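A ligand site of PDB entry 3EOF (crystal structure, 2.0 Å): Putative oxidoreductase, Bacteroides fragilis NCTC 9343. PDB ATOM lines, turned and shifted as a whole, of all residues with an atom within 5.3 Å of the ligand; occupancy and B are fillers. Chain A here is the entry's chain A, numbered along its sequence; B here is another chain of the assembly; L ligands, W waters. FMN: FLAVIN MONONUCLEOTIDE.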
ATOM      1  N   ARG A   9       3.019  -2.733  -2.373  1.00  0.00           N
ATOM      2  CA  ARG A   9       4.367  -3.123  -2.119  1.00  0.00           C
ATOM      3  C   ARG A   9       5.336  -2.554  -3.165  1.00  0.00           C
ATOM      4  O   ARG A   9       4.991  -2.254  -4.310  1.00  0.00           O
ATOM      5  CB  ARG A   9       4.532  -4.661  -2.028  1.00  0.00           C
ATOM      6  CG  ARG A   9       4.510  -5.412  -3.391  1.00  0.00           C
ATOM      7  CD  ARG A   9       5.144  -6.755  -3.335  1.00  0.00           C
ATOM      8  NE  ARG A   9       6.515  -6.646  -2.902  1.00  0.00           N
ATOM      9  CZ  ARG A   9       7.543  -6.334  -3.697  1.00  0.00           C
ATOM     10  NH1 ARG A   9       7.368  -6.135  -4.986  1.00  0.00           N
ATOM     11  NH2 ARG A   9       8.754  -6.241  -3.178  1.00  0.00           N
ATOM     12  N   ARG A  10       6.554  -2.386  -2.724  1.00  0.00           N
ATOM     13  CA  ARG A  10       7.604  -1.982  -3.587  1.00  0.00           C
ATOM     14  C   ARG A  10       8.878  -2.507  -2.967  1.00  0.00           C
ATOM     15  O   ARG A  10       8.948  -2.714  -1.749  1.00  0.00           O
ATOM     16  CB  ARG A  10       7.585  -0.464  -3.756  1.00  0.00           C
ATOM     17  CG  ARG A  10       7.824   0.297  -2.523  1.00  0.00           C
ATOM     18  CD  ARG A  10       7.105   1.589  -2.577  1.00  0.00           C
ATOM     19  NE  ARG A  10       5.678   1.415  -2.390  1.00  0.00           N
ATOM     20  CZ  ARG A  10       4.774   2.347  -2.679  1.00  0.00           C
ATOM     21  NH1 ARG A  10       5.140   3.517  -3.209  1.00  0.00           N
ATOM     22  NH2 ARG A  10       3.475   2.118  -2.480  1.00  0.00           N
ATOM     23  N   THR A  11       9.870  -2.700  -3.815  1.00  0.00           N
ATOM     24  CA  THR A  11      11.156  -3.176  -3.422  1.00  0.00           C
ATOM     25  C   THR A  11      11.868  -2.042  -2.663  1.00  0.00           C
ATOM     26  O   THR A  11      11.819  -0.892  -3.092  1.00  0.00           O
ATOM     27  CB  THR A  11      12.030  -3.633  -4.669  1.00  0.00           C
ATOM     28  OG1 THR A  11      11.529  -4.865  -5.191  1.00  0.00           O
ATOM     29  CG2 THR A  11      13.438  -3.878  -4.275  1.00  0.00           C
ATOM     30  N   ARG A  13      15.548  -0.935  -1.103  1.00  0.00           N
ATOM     31  CA  ARG A  13      16.975  -1.126  -1.241  1.00  0.00           C
ATOM     32  C   ARG A  13      17.826  -0.300  -0.274  1.00  0.00           C
ATOM     33  O   ARG A  13      19.047  -0.375  -0.300  1.00  0.00           O
ATOM     34  CB  ARG A  13      17.384  -0.749  -2.673  1.00  0.00           C
ATOM     35  CG  ARG A  13      16.784  -1.609  -3.749  1.00  0.00           C
ATOM     36  CD  ARG A  13      17.093  -1.080  -5.117  1.00  0.00           C
ATOM     37  NE  ARG A  13      16.593  -1.978  -6.164  1.00  0.00           N
ATOM     38  CZ  ARG A  13      15.372  -1.963  -6.681  1.00  0.00           C
ATOM     39  NH1 ARG A  13      14.435  -1.115  -6.282  1.00  0.00           N
ATOM     40  NH2 ARG A  13      15.053  -2.837  -7.627  1.00  0.00           N
ATOM     41  N   GLN A  65      26.317  -4.689  -5.221  1.00  0.00           N
ATOM     42  CA  GLN A  65      25.088  -3.929  -5.095  1.00  0.00           C
ATOM     43  C   GLN A  65      25.084  -3.590  -3.645  1.00  0.00           C
ATOM     44  O   GLN A  65      25.341  -4.457  -2.821  1.00  0.00           O
ATOM     45  CB  GLN A  65      23.881  -4.748  -5.451  1.00  0.00           C
ATOM     46  CG  GLN A  65      23.870  -5.191  -6.884  1.00  0.00           C
ATOM     47  CD  GLN A  65      22.625  -5.940  -7.220  1.00  0.00           C
ATOM     48  OE1 GLN A  65      21.588  -5.324  -7.406  1.00  0.00           O
ATOM     49  NE2 GLN A  65      22.711  -7.275  -7.297  1.00  0.00           N
ATOM     50  N   MET A  67      23.024  -3.086  -1.245  1.00  0.00           N
ATOM     51  CA  MET A  67      22.090  -3.680  -0.301  1.00  0.00           C
ATOM     52  C   MET A  67      22.667  -4.836   0.474  1.00  0.00           C
ATOM     53  O   MET A  67      22.204  -5.148   1.564  1.00  0.00           O
ATOM     54  CB  MET A  67      20.817  -4.188  -1.013  1.00  0.00           C
ATOM     55  CG  MET A  67      19.976  -3.152  -1.751  1.00  0.00           C
ATOM     56  SD  MET A  67      20.582  -2.692  -3.543  1.00  0.00           S
ATOM     57  CE  MET A  67      20.107  -4.312  -4.468  1.00  0.00           C
ATOM     58  N   CYS A 129      14.522  -6.885  -1.038  1.00  0.00           N
ATOM     59  CA  CYS A 129      14.997  -6.768  -2.396  1.00  0.00           C
ATOM     60  C   CYS A 129      15.610  -8.106  -2.746  1.00  0.00           C
ATOM     61  O   CYS A 129      16.420  -8.651  -1.990  1.00  0.00           O
ATOM     62  CB  CYS A 129      16.047  -5.686  -2.534  1.00  0.00           C
ATOM     63  SG  CYS A 129      16.575  -5.449  -4.221  1.00  0.00           S
ATOM     64  N   TYR A 130      15.204  -8.674  -3.875  1.00  0.00           N
ATOM     65  CA  TYR A 130      15.787  -9.913  -4.331  1.00  0.00           C
ATOM     66  C   TYR A 130      17.028  -9.528  -5.093  1.00  0.00           C
ATOM     67  O   TYR A 130      17.056  -8.476  -5.716  1.00  0.00           O
ATOM     68  CB  TYR A 130      14.855 -10.619  -5.291  1.00  0.00           C
ATOM     69  CG  TYR A 130      13.677 -11.380  -4.650  1.00  0.00           C
ATOM     70  CD1 TYR A 130      13.807 -12.710  -4.321  1.00  0.00           C
ATOM     71  CD2 TYR A 130      12.459 -10.802  -4.455  1.00  0.00           C
ATOM     72  CE1 TYR A 130      12.750 -13.459  -3.806  1.00  0.00           C
ATOM     73  CE2 TYR A 130      11.379 -11.537  -3.915  1.00  0.00           C
ATOM     74  CZ  TYR A 130      11.566 -12.896  -3.602  1.00  0.00           C
ATOM     75  OH  TYR A 130      10.576 -13.713  -3.060  1.00  0.00           O
ATOM     76  N   LEU A 131      18.046 -10.368  -5.045  1.00  0.00           N
ATOM     77  CA  LEU A 131      19.250 -10.178  -5.853  1.00  0.00           C
ATOM     78  C   LEU A 131      19.240 -11.357  -6.887  1.00  0.00           C
ATOM     79  O   LEU A 131      19.303 -12.600  -6.523  1.00  0.00           O
ATOM     80  CB  LEU A 131      20.529 -10.121  -5.017  1.00  0.00           C
ATOM     81  CG  LEU A 131      20.533  -9.300  -3.715  1.00  0.00           C
ATOM     82  CD1 LEU A 131      21.772  -9.667  -2.893  1.00  0.00           C
ATOM     83  CD2 LEU A 131      20.419  -7.770  -3.954  1.00  0.00           C
ATOM     84  N   GLY A 132      19.139 -10.932  -8.157  1.00  0.00           N
ATOM     85  CA  GLY A 132      19.146 -11.833  -9.317  1.00  0.00           C
ATOM     86  C   GLY A 132      20.540 -12.306  -9.636  1.00  0.00           C
ATOM     87  O   GLY A 132      20.773 -13.277 -10.414  1.00  0.00           O
ATOM     88  N   THR A 133      21.493 -11.628  -9.009  1.00  0.00           N
ATOM     89  CA  THR A 133      22.907 -11.959  -9.174  1.00  0.00           C
ATOM     90  C   THR A 133      23.292 -13.330  -8.616  1.00  0.00           C
ATOM     91  O   THR A 133      24.379 -13.855  -8.902  1.00  0.00           O
ATOM     92  CB  THR A 133      23.731 -10.851  -8.550  1.00  0.00           C
ATOM     93  OG1 THR A 133      23.146 -10.493  -7.282  1.00  0.00           O
ATOM     94  CG2 THR A 133      23.678  -9.638  -9.451  1.00  0.00           C
ATOM     95  N   THR A 155      18.015 -17.867  -4.808  1.00  0.00           N
ATOM     96  CA  THR A 155      17.955 -16.412  -4.763  1.00  0.00           C
ATOM     97  C   THR A 155      18.396 -15.882  -3.386  1.00  0.00           C
ATOM     98  O   THR A 155      18.517 -16.642  -2.439  1.00  0.00           O
ATOM     99  CB  THR A 155      16.612 -15.833  -5.136  1.00  0.00           C
ATOM    100  OG1 THR A 155      16.767 -14.411  -5.331  1.00  0.00           O
ATOM    101  CG2 THR A 155      15.606 -16.123  -4.056  1.00  0.00           C
ATOM    102  N   VAL A 169       6.710   1.007  -8.852  1.00  0.00           N
ATOM    103  CA  VAL A 169       6.920   0.852 -10.279  1.00  0.00           C
ATOM    104  C   VAL A 169       5.611   0.295 -10.893  1.00  0.00           C
ATOM    105  O   VAL A 169       4.736  -0.209 -10.204  1.00  0.00           O
ATOM    106  CB  VAL A 169       8.191   0.015 -10.643  1.00  0.00           C
ATOM    107  CG1 VAL A 169       9.328   0.289  -9.658  1.00  0.00           C
ATOM    108  CG2 VAL A 169       7.891  -1.384 -10.647  1.00  0.00           C
ATOM    109  N   ARG A 171       3.111  -1.980 -13.478  1.00  0.00           N
ATOM    110  CA  ARG A 171       2.868  -3.308 -13.930  1.00  0.00           C
ATOM    111  C   ARG A 171       1.982  -3.210 -15.173  1.00  0.00           C
ATOM    112  O   ARG A 171       1.275  -2.212 -15.381  1.00  0.00           O
ATOM    113  CB  ARG A 171       2.182  -4.124 -12.846  1.00  0.00           C
ATOM    114  CG  ARG A 171       3.102  -4.471 -11.686  1.00  0.00           C
ATOM    115  CD  ARG A 171       4.180  -5.404 -12.082  1.00  0.00           C
ATOM    116  NE  ARG A 171       4.858  -5.871 -10.889  1.00  0.00           N
ATOM    117  CZ  ARG A 171       5.863  -5.255 -10.275  1.00  0.00           C
ATOM    118  NH1 ARG A 171       6.401  -4.141 -10.745  1.00  0.00           N
ATOM    119  NH2 ARG A 171       6.339  -5.793  -9.174  1.00  0.00           N
ATOM    120  N   ARG B  34       2.103  -7.896  -8.347  1.00  0.00           N
ATOM    121  CA  ARG B  34       2.923  -6.944  -7.631  1.00  0.00           C
ATOM    122  C   ARG B  34       4.176  -7.555  -7.034  1.00  0.00           C
ATOM    123  O   ARG B  34       4.985  -6.853  -6.528  1.00  0.00           O
ATOM    124  CB  ARG B  34       2.078  -6.257  -6.526  1.00  0.00           C
ATOM    125  CG  ARG B  34       1.138  -5.200  -7.091  1.00  0.00           C
ATOM    126  CD  ARG B  34       2.012  -4.092  -7.641  1.00  0.00           C
ATOM    127  NE  ARG B  34       1.352  -3.054  -8.435  1.00  0.00           N
ATOM    128  CZ  ARG B  34       2.040  -2.132  -9.089  1.00  0.00           C
ATOM    129  NH1 ARG B  34       3.390  -2.106  -9.034  1.00  0.00           N
ATOM    130  NH2 ARG B  34       1.403  -1.208  -9.791  1.00  0.00           N
ATOM    131  N   ALA B  35       4.304  -8.877  -7.044  1.00  0.00           N
ATOM    132  CA  ALA B  35       5.471  -9.561  -6.548  1.00  0.00           C
ATOM    133  C   ALA B  35       6.644  -9.044  -7.333  1.00  0.00           C
ATOM    134  O   ALA B  35       6.438  -8.623  -8.447  1.00  0.00           O
ATOM    135  CB  ALA B  35       5.294 -11.094  -6.796  1.00  0.00           C
ATOM    136  N   SER B  36       7.850  -9.103  -6.759  1.00  0.00           N
ATOM    137  CA  SER B  36       9.087  -8.723  -7.454  1.00  0.00           C
ATOM    138  C   SER B  36       9.231  -9.444  -8.755  1.00  0.00           C
ATOM    139  O   SER B  36       8.839 -10.625  -8.885  1.00  0.00           O
ATOM    140  CB  SER B  36      10.314  -9.033  -6.612  1.00  0.00           C
ATOM    141  OG  SER B  36      10.123  -8.509  -5.297  1.00  0.00           O
ATOM    142  N   THR B  37       9.887  -8.776  -9.711  1.00  0.00           N
ATOM    143  CA  THR B  37      10.025  -9.311 -11.017  1.00  0.00           C
ATOM    144  C   THR B  37      11.305  -8.808 -11.623  1.00  0.00           C
ATOM    145  O   THR B  37      11.625  -7.629 -11.586  1.00  0.00           O
ATOM    146  CB  THR B  37       8.772  -9.002 -11.881  1.00  0.00           C
ATOM    147  OG1 THR B  37       9.076  -9.187 -13.246  1.00  0.00           O
ATOM    148  CG2 THR B  37       8.282  -7.565 -11.683  1.00  0.00           C
ATOM    149  N   MET B  38      12.098  -9.738 -12.122  1.00  0.00           N
ATOM    150  CA  MET B  38      13.353  -9.368 -12.716  1.00  0.00           C
ATOM    151  C   MET B  38      13.167  -8.224 -13.695  1.00  0.00           C
ATOM    152  O   MET B  38      12.430  -8.332 -14.664  1.00  0.00           O
ATOM    153  CB  MET B  38      13.960 -10.529 -13.446  1.00  0.00           C
ATOM    154  CG  MET B  38      15.384 -10.260 -13.813  1.00  0.00           C
ATOM    155  SD  MET B  38      16.191 -11.667 -14.762  1.00  0.00           S
ATOM    156  CE  MET B  38      15.749 -11.188 -16.653  1.00  0.00           C
ATOM    157  N   GLY B  39      13.835  -7.122 -13.408  1.00  0.00           N
ATOM    158  CA  GLY B  39      13.842  -5.961 -14.271  1.00  0.00           C
ATOM    159  C   GLY B  39      12.475  -5.337 -14.460  1.00  0.00           C
ATOM    160  O   GLY B  39      12.307  -4.551 -15.360  1.00  0.00           O
ATOM    161  N   GLY B  40      11.522  -5.665 -13.609  1.00  0.00           N
ATOM    162  CA  GLY B  40      10.135  -5.187 -13.782  1.00  0.00           C
ATOM    163  C   GLY B  40       9.484  -5.784 -15.020  1.00  0.00           C
ATOM    164  O   GLY B  40       8.474  -5.267 -15.496  1.00  0.00           O
ATOM    165  N   ASN B 105      15.220 -17.515 -15.009  1.00  0.00           N
ATOM    166  CA  ASN B 105      14.789 -16.166 -14.656  1.00  0.00           C
ATOM    167  C   ASN B 105      13.285 -16.041 -14.715  1.00  0.00           C
ATOM    168  O   ASN B 105      12.670 -15.580 -13.776  1.00  0.00           O
ATOM    169  CB  ASN B 105      15.470 -15.122 -15.582  1.00  0.00           C
ATOM    170  CG  ASN B 105      16.897 -14.888 -15.226  1.00  0.00           C
ATOM    171  OD1 ASN B 105      17.290 -15.082 -14.084  1.00  0.00           O
ATOM    172  ND2 ASN B 105      17.697 -14.409 -16.188  1.00  0.00           N
ATOM    173  N   MET B 108      11.494 -18.199 -11.943  1.00  0.00           N
ATOM    174  CA  MET B 108      11.543 -17.519 -10.618  1.00  0.00           C
ATOM    175  C   MET B 108      10.474 -16.438 -10.534  1.00  0.00           C
ATOM    176  O   MET B 108       9.670 -16.457  -9.615  1.00  0.00           O
ATOM    177  CB  MET B 108      12.945 -16.948 -10.398  1.00  0.00           C
ATOM    178  CG  MET B 108      13.961 -18.026 -10.244  1.00  0.00           C
ATOM    179  SD  MET B 108      15.677 -17.337  -9.556  1.00  0.00           S
ATOM    180  CE  MET B 108      16.281 -16.219 -11.079  1.00  0.00           C
ATOM    181  N   ASP B 109      10.404 -15.582 -11.541  1.00  0.00           N
ATOM    182  CA  ASP B 109       9.337 -14.587 -11.669  1.00  0.00           C
ATOM    183  C   ASP B 109       7.977 -15.273 -11.508  1.00  0.00           C
ATOM    184  O   ASP B 109       7.124 -14.822 -10.754  1.00  0.00           O
ATOM    185  CB  ASP B 109       9.349 -13.915 -13.057  1.00  0.00           C
ATOM    186  CG  ASP B 109      10.022 -12.561 -13.072  1.00  0.00           C
ATOM    187  OD1 ASP B 109      10.944 -12.300 -12.291  1.00  0.00           O
ATOM    188  OD2 ASP B 109       9.583 -11.713 -13.902  1.00  0.00           O
ATOM    189  N   LEU B 112       7.205 -16.716  -7.863  1.00  0.00           N
ATOM    190  CA  LEU B 112       6.957 -15.578  -6.961  1.00  0.00           C
ATOM    191  C   LEU B 112       5.529 -15.163  -7.106  1.00  0.00           C
ATOM    192  O   LEU B 112       4.852 -14.908  -6.106  1.00  0.00           O
ATOM    193  CB  LEU B 112       7.921 -14.396  -7.254  1.00  0.00           C
ATOM    194  CG  LEU B 112       9.266 -14.343  -6.522  1.00  0.00           C
ATOM    195  CD1 LEU B 112       9.952 -15.697  -6.259  1.00  0.00           C
ATOM    196  CD2 LEU B 112      10.260 -13.292  -7.187  1.00  0.00           C
HETATM  197  N1  FMN L   1      16.604  -5.485  -7.775  1.00  0.00           N
HETATM  198  C2  FMN L   1      17.916  -4.992  -7.775  1.00  0.00           C
HETATM  199  O2  FMN L   1      18.148  -3.813  -7.461  1.00  0.00           O
HETATM  200  N3  FMN L   1      18.991  -5.802  -8.153  1.00  0.00           N
HETATM  201  C4  FMN L   1      18.819  -7.142  -8.557  1.00  0.00           C
HETATM  202  O4  FMN L   1      19.822  -7.949  -8.484  1.00  0.00           O
HETATM  203  C4A FMN L   1      17.474  -7.619  -8.566  1.00  0.00           C
HETATM  204  N5  FMN L   1      17.223  -8.930  -8.951  1.00  0.00           N
HETATM  205  C5A FMN L   1      15.940  -9.463  -8.938  1.00  0.00           C
HETATM  206  C6  FMN L   1      15.788 -10.798  -9.328  1.00  0.00           C
HETATM  207  C7  FMN L   1      14.546 -11.395  -9.348  1.00  0.00           C
HETATM  208  C7M FMN L   1      14.457 -12.827  -9.802  1.00  0.00           C
HETATM  209  C8  FMN L   1      13.423 -10.650  -8.989  1.00  0.00           C
HETATM  210  C8M FMN L   1      12.131 -11.376  -8.792  1.00  0.00           C
HETATM  211  C9  FMN L   1      13.562  -9.303  -8.598  1.00  0.00           C
HETATM  212  C9A FMN L   1      14.833  -8.673  -8.559  1.00  0.00           C
HETATM  213  N10 FMN L   1      15.055  -7.322  -8.187  1.00  0.00           N
HETATM  214  C10 FMN L   1      16.363  -6.807  -8.186  1.00  0.00           C
HETATM  215  C1' FMN L   1      13.924  -6.364  -7.847  1.00  0.00           C
HETATM  216  C2' FMN L   1      13.219  -5.953  -9.138  1.00  0.00           C
HETATM  217  O2' FMN L   1      14.101  -5.086  -9.867  1.00  0.00           O
HETATM  218  C3' FMN L   1      11.854  -5.373  -8.872  1.00  0.00           C
HETATM  219  O3' FMN L   1      10.927  -6.341  -8.339  1.00  0.00           O
HETATM  220  C4' FMN L   1      11.217  -4.765 -10.125  1.00  0.00           C
HETATM  221  O4' FMN L   1      11.914  -3.594 -10.516  1.00  0.00           O
HETATM  222  C5' FMN L   1       9.816  -4.307  -9.821  1.00  0.00           C
HETATM  223  O5' FMN L   1       9.964  -3.469  -8.685  1.00  0.00           O
HETATM  224  P   FMN L   1       9.019  -3.645  -7.361  1.00  0.00           P
HETATM  225  O1P FMN L   1       9.285  -5.004  -6.684  1.00  0.00           O
HETATM  226  O2P FMN L   1       7.576  -3.599  -7.818  1.00  0.00           O
HETATM  227  O3P FMN L   1       9.299  -2.391  -6.520  1.00  0.00           O
HETATM  228  O   HOH W   1      12.800  -7.361  -5.012  1.00  0.00           O
HETATM  229  O   HOH W   2       7.488  -0.604  -6.960  1.00  0.00           O
HETATM  230  O   HOH W   3      12.000  -1.643  -8.309  1.00  0.00           O
HETATM  231  O   HOH W   4      16.139  -6.302 -11.525  1.00  0.00           O
HETATM  232  O   HOH W   5       5.378  -3.419  -6.782  1.00  0.00           O
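N of Thr 11 lies within hydrogen-bond range of O3P of the ligand (2.8 Å).
The side-chain hydroxyl (OG1) of Thr 11 lies within hydrogen-bond range of an oxygen (O1P) of the ligand (2.7 Å).
The guanidinium group (NE) of Arg 13 lies within hydrogen-bond range of an oxygen (O2) of the ligand (2.7 Å).
A nitrogen (N3) of the ligand lies within hydrogen-bond range of the side-chain amide oxygen of Gln 65, at 2.7 Å.
The guanidinium group (NH1) of Arg 9 is in salt-bridge range of an oxygen (O1P) of the ligand (2.8 Å).
O2P of the ligand is in salt-bridge range of NH2 of Arg 171 (2.9 Å).
A nitrogen (N5) of the ligand is in hydrogen-bond range of the backbone NH of Gly 132, 2.9 Å away.
N of Thr 37 of chain B is in hydrogen-bond range of O3' of the ligand (3.0 Å).
N1 of the ligand sits at hydrogen-bond distance from SG of Cys 129.
The side-chain hydroxyl of Ser 36 of chain B lies within hydrogen-bond range of the guanidinium group of Arg 9 (3.4 Å).
The guanidinium group (NH1) of Arg 9 is in hydrogen-bond range of the backbone carbonyl oxygen (O) of Arg 34 of chain B (2.9 Å).
The guanidinium group (NH2) of Arg 171 sits at hydrogen-bond distance from the backbone carbonyl oxygen (O) of Arg 34 of chain B, 3.2 Å away.
The guanidinium group of Arg 171 sits at hydrogen-bond distance from the backbone carbonyl oxygen of Ala 35 of chain B, at 2.9 Å.
The side-chain hydroxyl of Thr 155 lies within hydrogen-bond range of the backbone carbonyl oxygen of Leu 131, at 3.3 Å.
N of Met 38 of chain B is in hydrogen-bond range of OD1 of Asp 109 of chain B (2.8 Å).
ND2 of Asn 105 of chain B lies close to SD of Met 38 of chain B, at 3.4 Å.
NH1 of Arg 34 of chain B sits at hydrogen-bond distance from O of Val 169 (2.6 Å).
N5 of the ligand sits close to O of Tyr 130 (3.3 Å).
Arg 10 touches the ligand.
Met 67 touches the ligand.
Leu 131 touches the ligand (CA to O4, 3.5 Å).
Val 169 touches the ligand (CG2 to O5', 3.5 Å).
CA of Ser 36 of chain B touches O3' of the ligand, 3.1 Å away.
Met 38 of chain B touches the ligand.
Gly 40 of chain B touches the ligand (N to C4', 3.6 Å).
Asp 109 of chain B touches the ligand (OD1 to C8M, 3.8 Å).
Leu 112 of chain B touches the ligand.
Hydrophobic or aromatic side chains within 4 Å of the ligand: Met 67, Tyr 130, Val 169 and Leu 112 of chain B.
Of the 25 residues printed, 18 come within 4 Å of the ligand.
Water W5 lies within hydrogen-bond range of O2P of the ligand (2.4 Å), O of Arg 9 (2.8 Å) and NH1 of Arg 34 of chain B (3.3 Å).
Water W2 bridges O3P of the ligand (2.6 Å) and N of Val 169 (2.6 Å).
Water W3 lies within hydrogen-bond range of O5' of the ligand and NH1 of Arg 13.
Water W4 bridges O2' of the ligand (2.9 Å) and N of Gly 39 of chain B (3.1 Å).
Water W1 lies within hydrogen-bond range of OG1 of Thr 11 (2.8 Å), OG of Ser 36 of chain B (2.9 Å) and N of Tyr 130 (3.0 Å).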
